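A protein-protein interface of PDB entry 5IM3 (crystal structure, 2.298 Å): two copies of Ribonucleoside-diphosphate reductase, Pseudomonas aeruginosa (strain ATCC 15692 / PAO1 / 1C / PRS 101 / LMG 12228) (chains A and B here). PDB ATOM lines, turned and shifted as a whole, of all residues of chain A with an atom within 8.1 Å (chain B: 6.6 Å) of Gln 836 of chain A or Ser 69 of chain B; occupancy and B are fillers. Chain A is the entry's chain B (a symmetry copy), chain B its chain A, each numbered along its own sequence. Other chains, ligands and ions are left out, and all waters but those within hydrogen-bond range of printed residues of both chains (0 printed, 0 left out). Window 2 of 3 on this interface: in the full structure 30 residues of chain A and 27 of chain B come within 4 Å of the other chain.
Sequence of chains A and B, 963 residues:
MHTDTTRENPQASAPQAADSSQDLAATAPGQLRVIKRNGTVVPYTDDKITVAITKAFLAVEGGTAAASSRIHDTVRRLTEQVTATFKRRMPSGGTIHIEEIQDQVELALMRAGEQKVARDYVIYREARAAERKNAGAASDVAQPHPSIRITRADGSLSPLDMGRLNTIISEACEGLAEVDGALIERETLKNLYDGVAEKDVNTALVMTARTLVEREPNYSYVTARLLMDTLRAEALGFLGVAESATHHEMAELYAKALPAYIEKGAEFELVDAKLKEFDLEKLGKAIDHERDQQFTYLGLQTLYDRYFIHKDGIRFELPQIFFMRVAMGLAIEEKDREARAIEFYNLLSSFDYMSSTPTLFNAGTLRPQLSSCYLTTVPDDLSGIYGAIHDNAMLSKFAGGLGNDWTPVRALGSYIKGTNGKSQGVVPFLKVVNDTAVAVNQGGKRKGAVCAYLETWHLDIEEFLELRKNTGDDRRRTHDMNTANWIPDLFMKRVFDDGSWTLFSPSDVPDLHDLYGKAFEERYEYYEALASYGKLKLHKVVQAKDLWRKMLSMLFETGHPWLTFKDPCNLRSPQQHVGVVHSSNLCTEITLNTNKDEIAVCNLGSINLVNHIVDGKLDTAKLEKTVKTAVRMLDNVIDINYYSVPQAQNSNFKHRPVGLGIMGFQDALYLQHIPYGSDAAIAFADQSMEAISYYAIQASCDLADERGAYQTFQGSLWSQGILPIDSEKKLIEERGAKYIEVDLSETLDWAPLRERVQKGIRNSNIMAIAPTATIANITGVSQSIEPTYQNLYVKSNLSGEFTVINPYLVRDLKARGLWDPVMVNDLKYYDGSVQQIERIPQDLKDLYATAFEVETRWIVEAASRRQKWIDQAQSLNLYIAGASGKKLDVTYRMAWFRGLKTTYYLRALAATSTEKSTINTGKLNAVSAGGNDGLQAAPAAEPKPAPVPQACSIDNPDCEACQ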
ATOM      1  N   ASP A 826      25.680   8.076 -20.994  1.00  0.00           N
ATOM      2  CA  ASP A 826      25.846   7.272 -22.199  1.00  0.00           C
ATOM      3  C   ASP A 826      25.522   8.091 -23.439  1.00  0.00           C
ATOM      4  O   ASP A 826      26.241   8.024 -24.442  1.00  0.00           O
ATOM      5  CB  ASP A 826      24.968   6.019 -22.137  1.00  0.00           C
ATOM      6  CG  ASP A 826      25.568   4.924 -21.269  1.00  0.00           C
ATOM      7  OD1 ASP A 826      26.811   4.878 -21.129  1.00  0.00           O
ATOM      8  OD2 ASP A 826      24.795   4.102 -20.727  1.00  0.00           O
ATOM      9  N   TYR A 829      28.258  10.710 -24.064  1.00  0.00           N
ATOM     10  CA  TYR A 829      29.437  10.029 -24.593  1.00  0.00           C
ATOM     11  C   TYR A 829      29.294   9.736 -26.083  1.00  0.00           C
ATOM     12  O   TYR A 829      30.220   9.979 -26.865  1.00  0.00           O
ATOM     13  CB  TYR A 829      29.673   8.742 -23.804  1.00  0.00           C
ATOM     14  CG  TYR A 829      30.878   7.931 -24.232  1.00  0.00           C
ATOM     15  CD1 TYR A 829      32.163   8.301 -23.850  1.00  0.00           C
ATOM     16  CD2 TYR A 829      30.727   6.780 -24.992  1.00  0.00           C
ATOM     17  CE1 TYR A 829      33.262   7.554 -24.232  1.00  0.00           C
ATOM     18  CE2 TYR A 829      31.819   6.027 -25.375  1.00  0.00           C
ATOM     19  CZ  TYR A 829      33.085   6.419 -24.993  1.00  0.00           C
ATOM     20  OH  TYR A 829      34.174   5.670 -25.376  1.00  0.00           O
ATOM     21  N   TYR A 830      28.136   9.219 -26.498  1.00  0.00           N
ATOM     22  CA  TYR A 830      27.902   8.849 -27.889  1.00  0.00           C
ATOM     23  C   TYR A 830      27.290   9.975 -28.710  1.00  0.00           C
ATOM     24  O   TYR A 830      26.875   9.738 -29.848  1.00  0.00           O
ATOM     25  CB  TYR A 830      27.004   7.610 -27.961  1.00  0.00           C
ATOM     26  CG  TYR A 830      27.662   6.366 -27.416  1.00  0.00           C
ATOM     27  CD1 TYR A 830      28.707   5.756 -28.096  1.00  0.00           C
ATOM     28  CD2 TYR A 830      27.241   5.801 -26.219  1.00  0.00           C
ATOM     29  CE1 TYR A 830      29.316   4.620 -27.600  1.00  0.00           C
ATOM     30  CE2 TYR A 830      27.841   4.664 -25.718  1.00  0.00           C
ATOM     31  CZ  TYR A 830      28.879   4.078 -26.412  1.00  0.00           C
ATOM     32  OH  TYR A 830      29.486   2.946 -25.912  1.00  0.00           O
ATOM     33  N   SER A 833      23.725   9.309 -30.049  1.00  0.00           N
ATOM     34  CA  SER A 833      23.465   8.041 -30.709  1.00  0.00           C
ATOM     35  C   SER A 833      23.115   6.973 -29.682  1.00  0.00           C
ATOM     36  O   SER A 833      23.738   6.874 -28.621  1.00  0.00           O
ATOM     37  CB  SER A 833      24.677   7.604 -31.531  1.00  0.00           C
ATOM     38  OG  SER A 833      24.451   6.339 -32.127  1.00  0.00           O
ATOM     39  N   VAL A 834      22.103   6.172 -30.006  1.00  0.00           N
ATOM     40  CA  VAL A 834      21.641   5.085 -29.153  1.00  0.00           C
ATOM     41  C   VAL A 834      22.029   3.723 -29.696  1.00  0.00           C
ATOM     42  O   VAL A 834      21.648   2.700 -29.106  1.00  0.00           O
ATOM     43  CB  VAL A 834      20.114   5.156 -28.944  1.00  0.00           C
ATOM     44  CG1 VAL A 834      19.735   6.451 -28.228  1.00  0.00           C
ATOM     45  CG2 VAL A 834      19.378   5.053 -30.283  1.00  0.00           C
ATOM     46  N   GLN A 835      22.791   3.672 -30.793  1.00  0.00           N
ATOM     47  CA  GLN A 835      23.045   2.411 -31.478  1.00  0.00           C
ATOM     48  C   GLN A 835      23.955   1.484 -30.688  1.00  0.00           C
ATOM     49  O   GLN A 835      23.883   0.265 -30.879  1.00  0.00           O
ATOM     50  CB  GLN A 835      23.656   2.686 -32.856  1.00  0.00           C
ATOM     51  CG  GLN A 835      22.811   3.604 -33.727  1.00  0.00           C
ATOM     52  CD  GLN A 835      21.388   3.103 -33.884  1.00  0.00           C
ATOM     53  OE1 GLN A 835      21.160   1.923 -34.133  1.00  0.00           O
ATOM     54  NE2 GLN A 835      20.420   4.000 -33.718  1.00  0.00           N
ATOM     55  N   GLN A 836      24.793   2.021 -29.801  1.00  0.00           N
ATOM     56  CA  GLN A 836      25.756   1.225 -29.047  1.00  0.00           C
ATOM     57  C   GLN A 836      25.414   1.123 -27.564  1.00  0.00           C
ATOM     58  O   GLN A 836      26.273   0.728 -26.767  1.00  0.00           O
ATOM     59  CB  GLN A 836      27.159   1.810 -29.218  1.00  0.00           C
ATOM     60  CG  GLN A 836      27.643   1.829 -30.659  1.00  0.00           C
ATOM     61  CD  GLN A 836      28.850   2.727 -30.861  1.00  0.00           C
ATOM     62  OE1 GLN A 836      29.963   2.396 -30.452  1.00  0.00           O
ATOM     63  NE2 GLN A 836      28.632   3.874 -31.498  1.00  0.00           N
ATOM     64  N   ILE A 837      24.191   1.467 -27.173  1.00  0.00           N
ATOM     65  CA  ILE A 837      23.749   1.364 -25.786  1.00  0.00           C
ATOM     66  C   ILE A 837      22.941   0.077 -25.659  1.00  0.00           C
ATOM     67  O   ILE A 837      21.812  -0.011 -26.148  1.00  0.00           O
ATOM     68  CB  ILE A 837      22.931   2.592 -25.360  1.00  0.00           C
ATOM     69  CG1 ILE A 837      23.756   3.869 -25.552  1.00  0.00           C
ATOM     70  CG2 ILE A 837      22.490   2.456 -23.907  1.00  0.00           C
ATOM     71  CD1 ILE A 837      23.013   5.161 -25.215  1.00  0.00           C
ATOM     72  N   GLU A 838      23.515  -0.925 -24.990  1.00  0.00           N
ATOM     73  CA  GLU A 838      22.897  -2.249 -24.958  1.00  0.00           C
ATOM     74  C   GLU A 838      21.520  -2.227 -24.303  1.00  0.00           C
ATOM     75  O   GLU A 838      20.632  -2.990 -24.703  1.00  0.00           O
ATOM     76  CB  GLU A 838      23.804  -3.236 -24.221  1.00  0.00           C
ATOM     77  CG  GLU A 838      25.228  -3.315 -24.755  1.00  0.00           C
ATOM     78  CD  GLU A 838      26.194  -2.420 -23.992  1.00  0.00           C
ATOM     79  OE1 GLU A 838      26.087  -1.178 -24.123  1.00  0.00           O
ATOM     80  OE2 GLU A 838      27.051  -2.963 -23.253  1.00  0.00           O
ATOM     81  N   ARG A 839      21.324  -1.371 -23.297  1.00  0.00           N
ATOM     82  CA  ARG A 839      20.063  -1.350 -22.559  1.00  0.00           C
ATOM     83  C   ARG A 839      18.877  -0.979 -23.446  1.00  0.00           C
ATOM     84  O   ARG A 839      17.737  -1.342 -23.139  1.00  0.00           O
ATOM     85  CB  ARG A 839      20.157  -0.361 -21.397  1.00  0.00           C
ATOM     86  CG  ARG A 839      21.297  -0.633 -20.426  1.00  0.00           C
ATOM     87  CD  ARG A 839      21.576   0.587 -19.560  1.00  0.00           C
ATOM     88  NE  ARG A 839      20.424   0.961 -18.747  1.00  0.00           N
ATOM     89  CZ  ARG A 839      20.294   2.126 -18.121  1.00  0.00           C
ATOM     90  NH1 ARG A 839      21.241   3.052 -18.219  1.00  0.00           N
ATOM     91  NH2 ARG A 839      19.209   2.371 -17.397  1.00  0.00           N
ATOM     92  N   ILE A 840      19.113  -0.247 -24.529  1.00  0.00           N
ATOM     93  CA  ILE A 840      18.014   0.284 -25.331  1.00  0.00           C
ATOM     94  C   ILE A 840      17.524  -0.807 -26.282  1.00  0.00           C
ATOM     95  O   ILE A 840      18.324  -1.370 -27.041  1.00  0.00           O
ATOM     96  CB  ILE A 840      18.447   1.558 -26.073  1.00  0.00           C
ATOM     97  CG1 ILE A 840      18.769   2.648 -25.040  1.00  0.00           C
ATOM     98  CG2 ILE A 840      17.358   2.027 -27.041  1.00  0.00           C
ATOM     99  CD1 ILE A 840      19.145   3.998 -25.626  1.00  0.00           C
ATOM    100  N   LYS A 845      16.201   1.610 -31.004  1.00  0.00           N
ATOM    101  CA  LYS A 845      17.415   1.899 -31.760  1.00  0.00           C
ATOM    102  C   LYS A 845      17.078   2.310 -33.188  1.00  0.00           C
ATOM    103  O   LYS A 845      17.638   3.277 -33.713  1.00  0.00           O
ATOM    104  CB  LYS A 845      18.345   0.687 -31.761  1.00  0.00           C
ATOM    105  CG  LYS A 845      19.137   0.492 -30.474  1.00  0.00           C
ATOM    106  CD  LYS A 845      20.120  -0.665 -30.608  1.00  0.00           C
ATOM    107  CE  LYS A 845      21.000  -0.808 -29.379  1.00  0.00           C
ATOM    108  NZ  LYS A 845      20.234  -1.284 -28.200  1.00  0.00           N
ATOM    109  N   GLU A 853      22.761   7.891 -39.672  1.00  0.00           N
ATOM    110  CA  GLU A 853      22.529   6.482 -39.408  1.00  0.00           C
ATOM    111  C   GLU A 853      21.365   5.912 -40.207  1.00  0.00           C
ATOM    112  O   GLU A 853      21.196   4.689 -40.235  1.00  0.00           O
ATOM    113  CB  GLU A 853      22.284   6.268 -37.906  1.00  0.00           C
ATOM    114  CG  GLU A 853      23.417   6.805 -37.028  1.00  0.00           C
ATOM    115  CD  GLU A 853      23.081   6.797 -35.545  1.00  0.00           C
ATOM    116  OE1 GLU A 853      21.886   6.885 -35.198  1.00  0.00           O
ATOM    117  OE2 GLU A 853      24.018   6.706 -34.723  1.00  0.00           O
ATOM    118  N   ALA B  67      27.498  -2.719 -16.304  1.00  0.00           N
ATOM    119  CA  ALA B  67      27.468  -3.154 -17.698  1.00  0.00           C
ATOM    120  C   ALA B  67      27.221  -1.911 -18.546  1.00  0.00           C
ATOM    121  O   ALA B  67      26.081  -1.495 -18.759  1.00  0.00           O
ATOM    122  CB  ALA B  67      26.404  -4.221 -17.926  1.00  0.00           C
ATOM    123  N   SER B  68      28.306  -1.309 -19.023  1.00  0.00           N
ATOM    124  CA  SER B  68      28.223  -0.117 -19.858  1.00  0.00           C
ATOM    125  C   SER B  68      29.323  -0.188 -20.901  1.00  0.00           C
ATOM    126  O   SER B  68      30.509  -0.181 -20.554  1.00  0.00           O
ATOM    127  CB  SER B  68      28.359   1.161 -19.023  1.00  0.00           C
ATOM    128  OG  SER B  68      28.036   2.311 -19.789  1.00  0.00           O
ATOM    129  N   SER B  69      28.929  -0.268 -22.176  1.00  0.00           N
ATOM    130  CA  SER B  69      29.905  -0.186 -23.256  1.00  0.00           C
ATOM    131  C   SER B  69      30.752   1.072 -23.129  1.00  0.00           C
ATOM    132  O   SER B  69      31.930   1.071 -23.500  1.00  0.00           O
ATOM    133  CB  SER B  69      29.194  -0.211 -24.608  1.00  0.00           C
ATOM    134  OG  SER B  69      28.419   0.963 -24.791  1.00  0.00           O
ATOM    135  N   ARG B  70      30.172   2.150 -22.595  1.00  0.00           N
ATOM    136  CA  ARG B  70      30.903   3.402 -22.437  1.00  0.00           C
ATOM    137  C   ARG B  70      32.085   3.231 -21.491  1.00  0.00           C
ATOM    138  O   ARG B  70      33.243   3.443 -21.872  1.00  0.00           O
ATOM    139  CB  ARG B  70      29.955   4.488 -21.928  1.00  0.00           C
ATOM    140  CG  ARG B  70      30.651   5.747 -21.427  1.00  0.00           C
ATOM    141  CD  ARG B  70      29.638   6.791 -21.003  1.00  0.00           C
ATOM    142  NE  ARG B  70      28.713   6.279 -19.993  1.00  0.00           N
ATOM    143  CZ  ARG B  70      28.883   6.399 -18.679  1.00  0.00           C
ATOM    144  NH1 ARG B  70      29.948   7.020 -18.188  1.00  0.00           N
ATOM    145  NH2 ARG B  70      27.978   5.896 -17.849  1.00  0.00           N
ATOM    146  N   ILE B  71      31.807   2.859 -20.239  1.00  0.00           N
ATOM    147  CA  ILE B  71      32.871   2.683 -19.250  1.00  0.00           C
ATOM    148  C   ILE B  71      33.947   1.764 -19.810  1.00  0.00           C
ATOM    149  O   ILE B  71      35.128   2.121 -19.894  1.00  0.00           O
ATOM    150  CB  ILE B  71      32.304   2.118 -17.934  1.00  0.00           C
ATOM    151  CG1 ILE B  71      31.148   2.977 -17.400  1.00  0.00           C
ATOM    152  CG2 ILE B  71      33.414   2.002 -16.895  1.00  0.00           C
ATOM    153  CD1 ILE B  71      31.556   4.343 -16.904  1.00  0.00           C
ATOM    154  N   HIS B  72      33.534   0.563 -20.209  1.00  0.00           N
ATOM    155  CA  HIS B  72      34.470  -0.445 -20.693  1.00  0.00           C
ATOM    156  C   HIS B  72      35.287   0.069 -21.871  1.00  0.00           C
ATOM    157  O   HIS B  72      36.501  -0.157 -21.939  1.00  0.00           O
ATOM    158  CB  HIS B  72      33.678  -1.698 -21.058  1.00  0.00           C
ATOM    159  CG  HIS B  72      34.406  -2.655 -21.943  1.00  0.00           C
ATOM    160  ND1 HIS B  72      34.248  -2.664 -23.313  1.00  0.00           N
ATOM    161  CD2 HIS B  72      35.263  -3.663 -21.655  1.00  0.00           C
ATOM    162  CE1 HIS B  72      34.989  -3.626 -23.831  1.00  0.00           C
ATOM    163  NE2 HIS B  72      35.612  -4.249 -22.846  1.00  0.00           N
ATOM    164  N   ASP B  73      34.642   0.770 -22.806  1.00  0.00           N
ATOM    165  CA  ASP B  73      35.375   1.357 -23.923  1.00  0.00           C
ATOM    166  C   ASP B  73      36.359   2.415 -23.439  1.00  0.00           C
ATOM    167  O   ASP B  73      37.493   2.491 -23.927  1.00  0.00           O
ATOM    168  CB  ASP B  73      34.396   1.959 -24.933  1.00  0.00           C
ATOM    169  CG  ASP B  73      35.019   2.174 -26.297  1.00  0.00           C
ATOM    170  OD1 ASP B  73      35.975   1.446 -26.638  1.00  0.00           O
ATOM    171  OD2 ASP B  73      34.542   3.063 -27.034  1.00  0.00           O
ATOM    172  N   THR B  74      35.945   3.240 -22.476  1.00  0.00           N
ATOM    173  CA  THR B  74      36.814   4.298 -21.969  1.00  0.00           C
ATOM    174  C   THR B  74      37.999   3.721 -21.204  1.00  0.00           C
ATOM    175  O   THR B  74      39.148   4.108 -21.438  1.00  0.00           O
ATOM    176  CB  THR B  74      36.017   5.247 -21.073  1.00  0.00           C
ATOM    177  OG1 THR B  74      34.879   5.738 -21.788  1.00  0.00           O
ATOM    178  CG2 THR B  74      36.877   6.421 -20.633  1.00  0.00           C
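The backbone NH (N) of Arg 70 of chain B sits at hydrogen-bond distance from the side-chain hydroxyl (OH) of Tyr 830 of chain A (3.5 Å).
The side-chain hydroxyl of Ser 69 of chain B is in hydrogen-bond range of the backbone carbonyl oxygen of Gln 836 of chain A, at 2.9 Å.
The side-chain carboxylate (OD2) of Asp 73 of chain B sits at hydrogen-bond distance from the side-chain hydroxyl (OH) of Tyr 829 of chain A (3.1 Å).
OG of Ser 69 of chain B lies within hydrogen-bond range of OH of Tyr 830 of chain A, at 2.5 Å.
OD1 of Asp 826 of chain A lies within salt-bridge range of NE of Arg 70 of chain B, at 2.6 Å.
The side-chain hydroxyl (OG) of Ser 69 of chain B lies within hydrogen-bond range of the side-chain carboxylate (OE1) of Glu 838 of chain A (3.2 Å).
OD1 of Asp 826 of chain A sits at hydrogen-bond distance from OG of Ser 68 of chain B, at 3.1 Å.
The backbone carbonyl oxygen (O) of Arg 70 of chain B is in hydrogen-bond range of the side-chain hydroxyl (OG1) of Thr 74 of chain B, 2.8 Å away.
Among the printed residues, merely in contact across the chains: Tyr 829 of chain A with Arg 70 of chain B (3.4 Å) and Tyr 829 of chain A with Thr 74 of chain B (3.4 Å).
Printed residues of chain B within 4 Å of Asp 826 of chain A: Ser 68 (3.1 Å) and Arg 70 (2.6 Å).
Of the printed residues of chain B, Tyr 830 of chain A touches Ser 69 (2.5 Å) and Arg 70 (3.5 Å).
Gln 836 of chain A touches just one residue of chain B: Ser 69 (2.9 Å).
Ile 837 of chain A touches none of the printed residues of chain B.
Of the printed residues of chain B, Glu 838 of chain A touches Ser 69 (3.2 Å).
Of chain A, only Asp 826 (3.1 Å) comes within 4 Å of Ser 68 of chain B.
Of chain A, only Tyr 830 (2.5 Å), Gln 836 (2.9 Å) and Glu 838 (3.2 Å) come within 4 Å of Ser 69 of chain B.
Of the printed residues of chain A, Arg 70 of chain B touches Asp 826 (2.6 Å), Tyr 829 (3.4 Å) and Tyr 830 (3.5 Å).
Printed residues of chain A within 4 Å of Thr 74 of chain B: Tyr 829 (3.4 Å).
Hydrophobic or aromatic side chains of chain A that line the printed part of chain B: Tyr 829 and Tyr 830.
Among the printed residues, 9 pairs touch across the chains.
Among the printed residues, Asp or Glu carboxylates within 4 Å of a Lys or Arg side-chain nitrogen of the other chain: Asp 826 of chain A with Arg 70 of chain B.
No position is printed for both chains.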
